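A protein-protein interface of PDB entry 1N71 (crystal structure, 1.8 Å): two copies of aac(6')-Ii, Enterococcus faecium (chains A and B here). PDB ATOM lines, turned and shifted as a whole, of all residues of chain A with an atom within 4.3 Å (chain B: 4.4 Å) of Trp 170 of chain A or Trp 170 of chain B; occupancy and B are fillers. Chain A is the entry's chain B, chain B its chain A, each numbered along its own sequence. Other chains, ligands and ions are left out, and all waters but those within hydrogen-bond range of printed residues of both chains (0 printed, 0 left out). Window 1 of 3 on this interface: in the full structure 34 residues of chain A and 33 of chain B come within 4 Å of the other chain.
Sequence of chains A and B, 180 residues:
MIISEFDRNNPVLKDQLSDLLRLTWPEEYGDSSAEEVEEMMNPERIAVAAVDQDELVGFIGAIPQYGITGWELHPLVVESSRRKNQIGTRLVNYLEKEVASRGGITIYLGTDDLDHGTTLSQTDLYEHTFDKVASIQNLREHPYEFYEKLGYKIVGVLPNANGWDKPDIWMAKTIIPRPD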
ATOM      1  N   TYR A 108     -11.009  20.526  -8.956  1.00  0.00           N
ATOM      2  CA  TYR A 108     -11.147  21.742  -8.162  1.00  0.00           C
ATOM      3  C   TYR A 108     -12.418  22.460  -8.581  1.00  0.00           C
ATOM      4  O   TYR A 108     -13.021  22.129  -9.600  1.00  0.00           O
ATOM      5  CB  TYR A 108      -9.949  22.674  -8.346  1.00  0.00           C
ATOM      6  CG  TYR A 108      -9.866  23.295  -9.720  1.00  0.00           C
ATOM      7  CD1 TYR A 108      -9.510  22.530 -10.826  1.00  0.00           C
ATOM      8  CD2 TYR A 108     -10.165  24.646  -9.916  1.00  0.00           C
ATOM      9  CE1 TYR A 108      -9.450  23.082 -12.100  1.00  0.00           C
ATOM     10  CE2 TYR A 108     -10.112  25.213 -11.191  1.00  0.00           C
ATOM     11  CZ  TYR A 108      -9.753  24.420 -12.276  1.00  0.00           C
ATOM     12  OH  TYR A 108      -9.698  24.949 -13.541  1.00  0.00           O
ATOM     13  N   LEU A 109     -12.826  23.437  -7.787  1.00  0.00           N
ATOM     14  CA  LEU A 109     -14.028  24.190  -8.086  1.00  0.00           C
ATOM     15  C   LEU A 109     -13.968  25.536  -7.390  1.00  0.00           C
ATOM     16  O   LEU A 109     -13.168  25.744  -6.477  1.00  0.00           O
ATOM     17  CB  LEU A 109     -15.259  23.416  -7.604  1.00  0.00           C
ATOM     18  CG  LEU A 109     -15.214  23.076  -6.107  1.00  0.00           C
ATOM     19  CD1 LEU A 109     -16.078  24.070  -5.327  1.00  0.00           C
ATOM     20  CD2 LEU A 109     -15.695  21.647  -5.887  1.00  0.00           C
ATOM     21  N   GLY A 110     -14.807  26.451  -7.854  1.00  0.00           N
ATOM     22  CA  GLY A 110     -14.893  27.766  -7.260  1.00  0.00           C
ATOM     23  C   GLY A 110     -16.338  27.937  -6.832  1.00  0.00           C
ATOM     24  O   GLY A 110     -17.257  27.799  -7.643  1.00  0.00           O
ATOM     25  N   LYS A 153     -10.964  20.472   0.063  1.00  0.00           N
ATOM     26  CA  LYS A 153     -10.374  21.416   1.002  1.00  0.00           C
ATOM     27  C   LYS A 153     -10.245  22.802   0.381  1.00  0.00           C
ATOM     28  O   LYS A 153      -9.935  22.934  -0.803  1.00  0.00           O
ATOM     29  CB  LYS A 153      -8.977  20.932   1.428  1.00  0.00           C
ATOM     30  CG  LYS A 153      -8.237  21.877   2.381  1.00  0.00           C
ATOM     31  CD  LYS A 153      -6.824  21.368   2.695  1.00  0.00           C
ATOM     32  CE  LYS A 153      -6.114  22.272   3.699  1.00  0.00           C
ATOM     33  NZ  LYS A 153      -4.768  21.749   4.089  1.00  0.00           N
ATOM     34  N   ILE A 154     -10.489  23.837   1.176  1.00  0.00           N
ATOM     35  CA  ILE A 154     -10.334  25.191   0.667  1.00  0.00           C
ATOM     36  C   ILE A 154      -8.832  25.380   0.461  1.00  0.00           C
ATOM     37  O   ILE A 154      -8.040  25.280   1.410  1.00  0.00           O
ATOM     38  CB  ILE A 154     -10.851  26.243   1.661  1.00  0.00           C
ATOM     39  CG1 ILE A 154     -12.350  26.041   1.900  1.00  0.00           C
ATOM     40  CG2 ILE A 154     -10.607  27.640   1.107  1.00  0.00           C
ATOM     41  CD1 ILE A 154     -12.900  26.901   3.025  1.00  0.00           C
ATOM     42  N   VAL A 155      -8.438  25.622  -0.785  1.00  0.00           N
ATOM     43  CA  VAL A 155      -7.033  25.813  -1.109  1.00  0.00           C
ATOM     44  C   VAL A 155      -6.735  27.230  -1.599  1.00  0.00           C
ATOM     45  O   VAL A 155      -5.600  27.555  -1.950  1.00  0.00           O
ATOM     46  CB  VAL A 155      -6.563  24.799  -2.172  1.00  0.00           C
ATOM     47  CG1 VAL A 155      -6.504  23.401  -1.560  1.00  0.00           C
ATOM     48  CG2 VAL A 155      -7.512  24.806  -3.367  1.00  0.00           C
ATOM     49  N   GLY A 156      -7.762  28.071  -1.613  1.00  0.00           N
ATOM     50  CA  GLY A 156      -7.567  29.440  -2.039  1.00  0.00           C
ATOM     51  C   GLY A 156      -8.833  30.268  -2.026  1.00  0.00           C
ATOM     52  O   GLY A 156      -9.936  29.745  -1.884  1.00  0.00           O
ATOM     53  N   VAL A 157      -8.665  31.578  -2.156  1.00  0.00           N
ATOM     54  CA  VAL A 157      -9.793  32.493  -2.201  1.00  0.00           C
ATOM     55  C   VAL A 157      -9.455  33.634  -3.145  1.00  0.00           C
ATOM     56  O   VAL A 157      -8.289  33.999  -3.298  1.00  0.00           O
ATOM     57  CB  VAL A 157     -10.112  33.093  -0.811  1.00  0.00           C
ATOM     58  CG1 VAL A 157     -10.579  32.004   0.128  1.00  0.00           C
ATOM     59  CG2 VAL A 157      -8.874  33.797  -0.242  1.00  0.00           C
ATOM     60  N   LEU A 158     -10.469  34.181  -3.799  1.00  0.00           N
ATOM     61  CA  LEU A 158     -10.256  35.312  -4.692  1.00  0.00           C
ATOM     62  C   LEU A 158     -11.055  36.463  -4.099  1.00  0.00           C
ATOM     63  O   LEU A 158     -12.263  36.549  -4.287  1.00  0.00           O
ATOM     64  CB  LEU A 158     -10.752  35.000  -6.104  1.00  0.00           C
ATOM     65  CG  LEU A 158     -10.623  36.158  -7.097  1.00  0.00           C
ATOM     66  CD1 LEU A 158      -9.197  36.708  -7.101  1.00  0.00           C
ATOM     67  CD2 LEU A 158     -11.026  35.669  -8.479  1.00  0.00           C
ATOM     68  N   ASP A 168     -14.743  34.416  -4.216  1.00  0.00           N
ATOM     69  CA  ASP A 168     -14.953  33.101  -4.797  1.00  0.00           C
ATOM     70  C   ASP A 168     -14.055  32.255  -3.896  1.00  0.00           C
ATOM     71  O   ASP A 168     -12.982  32.704  -3.474  1.00  0.00           O
ATOM     72  CB  ASP A 168     -14.473  33.039  -6.256  1.00  0.00           C
ATOM     73  CG  ASP A 168     -14.885  31.738  -6.959  1.00  0.00           C
ATOM     74  OD1 ASP A 168     -15.785  31.038  -6.458  1.00  0.00           O
ATOM     75  OD2 ASP A 168     -14.315  31.415  -8.026  1.00  0.00           O
ATOM     76  N   ILE A 169     -14.503  31.053  -3.567  1.00  0.00           N
ATOM     77  CA  ILE A 169     -13.739  30.168  -2.700  1.00  0.00           C
ATOM     78  C   ILE A 169     -13.312  28.958  -3.511  1.00  0.00           C
ATOM     79  O   ILE A 169     -14.161  28.228  -4.022  1.00  0.00           O
ATOM     80  CB  ILE A 169     -14.597  29.705  -1.497  1.00  0.00           C
ATOM     81  CG1 ILE A 169     -15.080  30.925  -0.710  1.00  0.00           C
ATOM     82  CG2 ILE A 169     -13.787  28.797  -0.589  1.00  0.00           C
ATOM     83  CD1 ILE A 169     -15.975  30.585   0.465  1.00  0.00           C
ATOM     84  N   TRP A 170     -12.002  28.758  -3.626  1.00  0.00           N
ATOM     85  CA  TRP A 170     -11.454  27.640  -4.393  1.00  0.00           C
ATOM     86  C   TRP A 170     -11.264  26.410  -3.523  1.00  0.00           C
ATOM     87  O   TRP A 170     -10.647  26.486  -2.459  1.00  0.00           O
ATOM     88  CB  TRP A 170     -10.098  28.015  -4.997  1.00  0.00           C
ATOM     89  CG  TRP A 170     -10.164  28.774  -6.286  1.00  0.00           C
ATOM     90  CD1 TRP A 170     -10.813  28.396  -7.427  1.00  0.00           C
ATOM     91  CD2 TRP A 170      -9.498  30.006  -6.592  1.00  0.00           C
ATOM     92  NE1 TRP A 170     -10.587  29.315  -8.427  1.00  0.00           N
ATOM     93  CE2 TRP A 170      -9.785  30.313  -7.940  1.00  0.00           C
ATOM     94  CE3 TRP A 170      -8.684  30.878  -5.858  1.00  0.00           C
ATOM     95  CZ2 TRP A 170      -9.287  31.462  -8.571  1.00  0.00           C
ATOM     96  CZ3 TRP A 170      -8.187  32.023  -6.487  1.00  0.00           C
ATOM     97  CH2 TRP A 170      -8.493  32.300  -7.831  1.00  0.00           C
ATOM     98  N   MET A 171     -11.779  25.279  -3.990  1.00  0.00           N
ATOM     99  CA  MET A 171     -11.660  24.030  -3.255  1.00  0.00           C
ATOM    100  C   MET A 171     -11.108  22.969  -4.186  1.00  0.00           C
ATOM    101  O   MET A 171     -11.295  23.043  -5.396  1.00  0.00           O
ATOM    102  CB  MET A 171     -13.027  23.619  -2.720  1.00  0.00           C
ATOM    103  CG  MET A 171     -13.667  24.710  -1.877  1.00  0.00           C
ATOM    104  SD  MET A 171     -15.185  24.167  -1.114  1.00  0.00           S
ATOM    105  CE  MET A 171     -14.519  23.049   0.131  1.00  0.00           C
ATOM    106  N   TYR B 108      -6.825  38.399 -11.394  1.00  0.00           N
ATOM    107  CA  TYR B 108      -6.160  37.236 -10.829  1.00  0.00           C
ATOM    108  C   TYR B 108      -5.530  36.456 -11.970  1.00  0.00           C
ATOM    109  O   TYR B 108      -5.858  36.668 -13.134  1.00  0.00           O
ATOM    110  CB  TYR B 108      -7.151  36.348 -10.073  1.00  0.00           C
ATOM    111  CG  TYR B 108      -8.121  35.622 -10.968  1.00  0.00           C
ATOM    112  CD1 TYR B 108      -9.238  36.274 -11.499  1.00  0.00           C
ATOM    113  CD2 TYR B 108      -7.917  34.282 -11.297  1.00  0.00           C
ATOM    114  CE1 TYR B 108     -10.128  35.605 -12.332  1.00  0.00           C
ATOM    115  CE2 TYR B 108      -8.799  33.605 -12.131  1.00  0.00           C
ATOM    116  CZ  TYR B 108      -9.900  34.270 -12.642  1.00  0.00           C
ATOM    117  OH  TYR B 108     -10.773  33.598 -13.461  1.00  0.00           O
ATOM    118  N   LEU B 109      -4.626  35.550 -11.629  1.00  0.00           N
ATOM    119  CA  LEU B 109      -3.928  34.760 -12.627  1.00  0.00           C
ATOM    120  C   LEU B 109      -3.453  33.457 -12.013  1.00  0.00           C
ATOM    121  O   LEU B 109      -3.411  33.307 -10.789  1.00  0.00           O
ATOM    122  CB  LEU B 109      -2.719  35.547 -13.147  1.00  0.00           C
ATOM    123  CG  LEU B 109      -1.711  35.939 -12.055  1.00  0.00           C
ATOM    124  CD1 LEU B 109      -0.682  34.823 -11.866  1.00  0.00           C
ATOM    125  CD2 LEU B 109      -1.011  37.235 -12.436  1.00  0.00           C
ATOM    126  N   GLY B 110      -3.116  32.512 -12.878  1.00  0.00           N
ATOM    127  CA  GLY B 110      -2.605  31.238 -12.423  1.00  0.00           C
ATOM    128  C   GLY B 110      -1.246  31.045 -13.070  1.00  0.00           C
ATOM    129  O   GLY B 110      -1.131  31.073 -14.298  1.00  0.00           O
ATOM    130  N   LYS B 153      -0.609  39.091  -4.937  1.00  0.00           N
ATOM    131  CA  LYS B 153      -0.341  38.230  -3.792  1.00  0.00           C
ATOM    132  C   LYS B 153      -0.798  36.809  -4.081  1.00  0.00           C
ATOM    133  O   LYS B 153      -1.789  36.608  -4.771  1.00  0.00           O
ATOM    134  CB  LYS B 153      -1.091  38.788  -2.575  1.00  0.00           C
ATOM    135  CG  LYS B 153      -1.339  37.814  -1.436  1.00  0.00           C
ATOM    136  CD  LYS B 153      -2.126  38.498  -0.309  1.00  0.00           C
ATOM    137  CE  LYS B 153      -2.334  37.568   0.877  1.00  0.00           C
ATOM    138  NZ  LYS B 153      -2.831  38.299   2.083  1.00  0.00           N
ATOM    139  N   ILE B 154      -0.076  35.818  -3.571  1.00  0.00           N
ATOM    140  CA  ILE B 154      -0.508  34.441  -3.776  1.00  0.00           C
ATOM    141  C   ILE B 154      -1.699  34.256  -2.849  1.00  0.00           C
ATOM    142  O   ILE B 154      -1.575  34.408  -1.629  1.00  0.00           O
ATOM    143  CB  ILE B 154       0.584  33.419  -3.396  1.00  0.00           C
ATOM    144  CG1 ILE B 154       1.812  33.610  -4.297  1.00  0.00           C
ATOM    145  CG2 ILE B 154       0.020  31.989  -3.527  1.00  0.00           C
ATOM    146  CD1 ILE B 154       3.025  32.744  -3.915  1.00  0.00           C
ATOM    147  N   VAL B 155      -2.852  33.936  -3.427  1.00  0.00           N
ATOM    148  CA  VAL B 155      -4.074  33.749  -2.654  1.00  0.00           C
ATOM    149  C   VAL B 155      -4.589  32.320  -2.720  1.00  0.00           C
ATOM    150  O   VAL B 155      -5.654  32.011  -2.192  1.00  0.00           O
ATOM    151  CB  VAL B 155      -5.192  34.673  -3.148  1.00  0.00           C
ATOM    152  CG1 VAL B 155      -4.819  36.125  -2.886  1.00  0.00           C
ATOM    153  CG2 VAL B 155      -5.434  34.444  -4.640  1.00  0.00           C
ATOM    154  N   GLY B 156      -3.843  31.446  -3.379  1.00  0.00           N
ATOM    155  CA  GLY B 156      -4.279  30.066  -3.454  1.00  0.00           C
ATOM    156  C   GLY B 156      -3.364  29.208  -4.293  1.00  0.00           C
ATOM    157  O   GLY B 156      -2.504  29.721  -5.010  1.00  0.00           O
ATOM    158  N   VAL B 157      -3.549  27.896  -4.189  1.00  0.00           N
ATOM    159  CA  VAL B 157      -2.772  26.934  -4.953  1.00  0.00           C
ATOM    160  C   VAL B 157      -3.680  25.784  -5.364  1.00  0.00           C
ATOM    161  O   VAL B 157      -4.671  25.493  -4.699  1.00  0.00           O
ATOM    162  CB  VAL B 157      -1.584  26.339  -4.140  1.00  0.00           C
ATOM    163  CG1 VAL B 157      -0.547  27.423  -3.854  1.00  0.00           C
ATOM    164  CG2 VAL B 157      -2.094  25.709  -2.840  1.00  0.00           C
ATOM    165  N   LEU B 158      -3.342  25.148  -6.475  1.00  0.00           N
ATOM    166  CA  LEU B 158      -4.104  24.013  -6.972  1.00  0.00           C
ATOM    167  C   LEU B 158      -3.151  22.823  -6.933  1.00  0.00           C
ATOM    168  O   LEU B 158      -2.363  22.609  -7.855  1.00  0.00           O
ATOM    169  CB  LEU B 158      -4.575  24.274  -8.399  1.00  0.00           C
ATOM    170  CG  LEU B 158      -5.409  23.163  -9.037  1.00  0.00           C
ATOM    171  CD1 LEU B 158      -6.465  22.663  -8.056  1.00  0.00           C
ATOM    172  CD2 LEU B 158      -6.047  23.696 -10.311  1.00  0.00           C
ATOM    173  N   ASP B 168      -0.570  24.727  -9.620  1.00  0.00           N
ATOM    174  CA  ASP B 168      -0.809  25.995 -10.278  1.00  0.00           C
ATOM    175  C   ASP B 168      -0.841  26.921  -9.068  1.00  0.00           C
ATOM    176  O   ASP B 168      -1.328  26.537  -8.002  1.00  0.00           O
ATOM    177  CB  ASP B 168      -2.156  26.024 -11.014  1.00  0.00           C
ATOM    178  CG  ASP B 168      -2.296  27.248 -11.926  1.00  0.00           C
ATOM    179  OD1 ASP B 168      -1.264  27.881 -12.232  1.00  0.00           O
ATOM    180  OD2 ASP B 168      -3.428  27.570 -12.348  1.00  0.00           O
ATOM    181  N   ILE B 169      -0.285  28.116  -9.214  1.00  0.00           N
ATOM    182  CA  ILE B 169      -0.257  29.080  -8.125  1.00  0.00           C
ATOM    183  C   ILE B 169      -1.181  30.233  -8.504  1.00  0.00           C
ATOM    184  O   ILE B 169      -0.976  30.868  -9.536  1.00  0.00           O
ATOM    185  CB  ILE B 169       1.167  29.627  -7.918  1.00  0.00           C
ATOM    186  CG1 ILE B 169       2.123  28.471  -7.591  1.00  0.00           C
ATOM    187  CG2 ILE B 169       1.170  30.662  -6.803  1.00  0.00           C
ATOM    188  CD1 ILE B 169       3.608  28.856  -7.605  1.00  0.00           C
ATOM    189  N   TRP B 170      -2.195  30.489  -7.679  1.00  0.00           N
ATOM    190  CA  TRP B 170      -3.151  31.566  -7.940  1.00  0.00           C
ATOM    191  C   TRP B 170      -2.736  32.861  -7.252  1.00  0.00           C
ATOM    192  O   TRP B 170      -2.508  32.884  -6.045  1.00  0.00           O
ATOM    193  CB  TRP B 170      -4.552  31.182  -7.449  1.00  0.00           C
ATOM    194  CG  TRP B 170      -5.317  30.275  -8.358  1.00  0.00           C
ATOM    195  CD1 TRP B 170      -5.614  30.489  -9.677  1.00  0.00           C
ATOM    196  CD2 TRP B 170      -5.956  29.043  -7.999  1.00  0.00           C
ATOM    197  NE1 TRP B 170      -6.404  29.471 -10.157  1.00  0.00           N
ATOM    198  CE2 TRP B 170      -6.628  28.570  -9.148  1.00  0.00           C
ATOM    199  CE3 TRP B 170      -6.030  28.296  -6.815  1.00  0.00           C
ATOM    200  CZ2 TRP B 170      -7.365  27.381  -9.151  1.00  0.00           C
ATOM    201  CZ3 TRP B 170      -6.765  27.112  -6.816  1.00  0.00           C
ATOM    202  CH2 TRP B 170      -7.423  26.667  -7.980  1.00  0.00           C
ATOM    203  N   MET B 171      -2.659  33.938  -8.026  1.00  0.00           N
ATOM    204  CA  MET B 171      -2.283  35.240  -7.501  1.00  0.00           C
ATOM    205  C   MET B 171      -3.355  36.266  -7.859  1.00  0.00           C
ATOM    206  O   MET B 171      -4.029  36.145  -8.882  1.00  0.00           O
ATOM    207  CB  MET B 171      -0.936  35.663  -8.075  1.00  0.00           C
ATOM    208  CG  MET B 171       0.165  34.642  -7.822  1.00  0.00           C
ATOM    209  SD  MET B 171       1.781  35.232  -8.286  1.00  0.00           S
ATOM    210  CE  MET B 171       2.022  36.532  -7.084  1.00  0.00           C
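N of Val 155 of chain B is in hydrogen-bond range of O of Trp 170 of chain B (2.8 Å). The backbone carbonyl oxygen of Gly 156 of chain B lies within hydrogen-bond range of the backbone NH of Trp 170 of chain B, 2.8 Å away. N of Leu 158 of chain B is in hydrogen-bond range of O of Asp 168 of chain B (2.9 Å). O of Trp 170 of chain A is in hydrogen-bond range of N of Val 155 of chain A. The backbone carbonyl oxygen (O) of Gly 156 of chain A sits at hydrogen-bond distance from the backbone NH (N) of Trp 170 of chain A. O of Asp 168 of chain A lies within hydrogen-bond range of N of Leu 158 of chain A (2.9 Å).
O of Val 155 of chain B is in hydrogen-bond range of N of Val 157 of chain A (3.0 Å). N of Val 157 of chain B is in hydrogen-bond range of O of Val 155 of chain A (3.1 Å).
Printed residues of chain B within 4 Å of Tyr 108 of chain A: Leu 158 (3.5 Å) and Trp 170 (3.9 Å). Printed residues of chain B within 4 Å of Val 155 of chain A: Gly 156 (3.2 Å) and Val 157 (3.1 Å). Printed residues of chain B within 4 Å of Leu 158 of chain A: Tyr 108 (3.6 Å). Trp 170 of chain A touches just one residue of chain B: Trp 170. Of the printed residues of chain A, Tyr 108 of chain B touches Leu 158. Printed residues of chain A within 4 Å of Trp 170 of chain B: Tyr 108 and Trp 170. The nearest residue of chain B that does not touch Trp 170 of chain A is Tyr 108 of chain B (4.03 Å). The nearest residue of chain A that does not touch Trp 170 of chain B is Val 155 of chain A (4.2 Å).
Among the printed residues, pairs that only touch across the chains: Gly 156 of chain A with Val 155 of chain B (3.2 Å), Val 155 of chain A with Gly 156 of chain B (3.2 Å), Tyr 108 of chain A with Leu 158 of chain B (3.5 Å), Leu 158 of chain A with Tyr 108 of chain B (3.6 Å), Gly 156 of chain A with Gly 156 of chain B (3.6 Å), Trp 170 of chain A with Trp 170 of chain B (3.8 Å) and Tyr 108 of chain A with Trp 170 of chain B (3.9 Å).
Tyr 108 of chain A touches Trp 170 of chain B, but with the chains exchanged Trp 170 of chain A does not touch Tyr 108 of chain B (4.03 Å). Val 155 of chain A touches Gly 156 of chain B, and with the chains exchanged Gly 156 of chain A touches Val 155 of chain B. Gly 156 of chain B touches its own counterpart, Gly 156 of chain A. Trp 170 of chain A touches its own counterpart, Trp 170 of chain B. 13 positions are printed for both chains. Of the 9 pairs that touch across the chains among the printed residues, 8 have their exchanged pair printed and touching as well.
Of the 13 printed residues of chain A, 6 touch a printed residue of chain B. Printed residues of chain A that touch a printed residue of chain B: Tyr 108, Val 155, Gly 156, Val 157, Leu 158 and Trp 170. Of the 13 printed residues of chain B, 6 touch a printed residue of chain A. Hydrophobic or aromatic side chains of chain B that line the printed part of chain A: Tyr 108, Val 155, Leu 158 and Trp 170.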
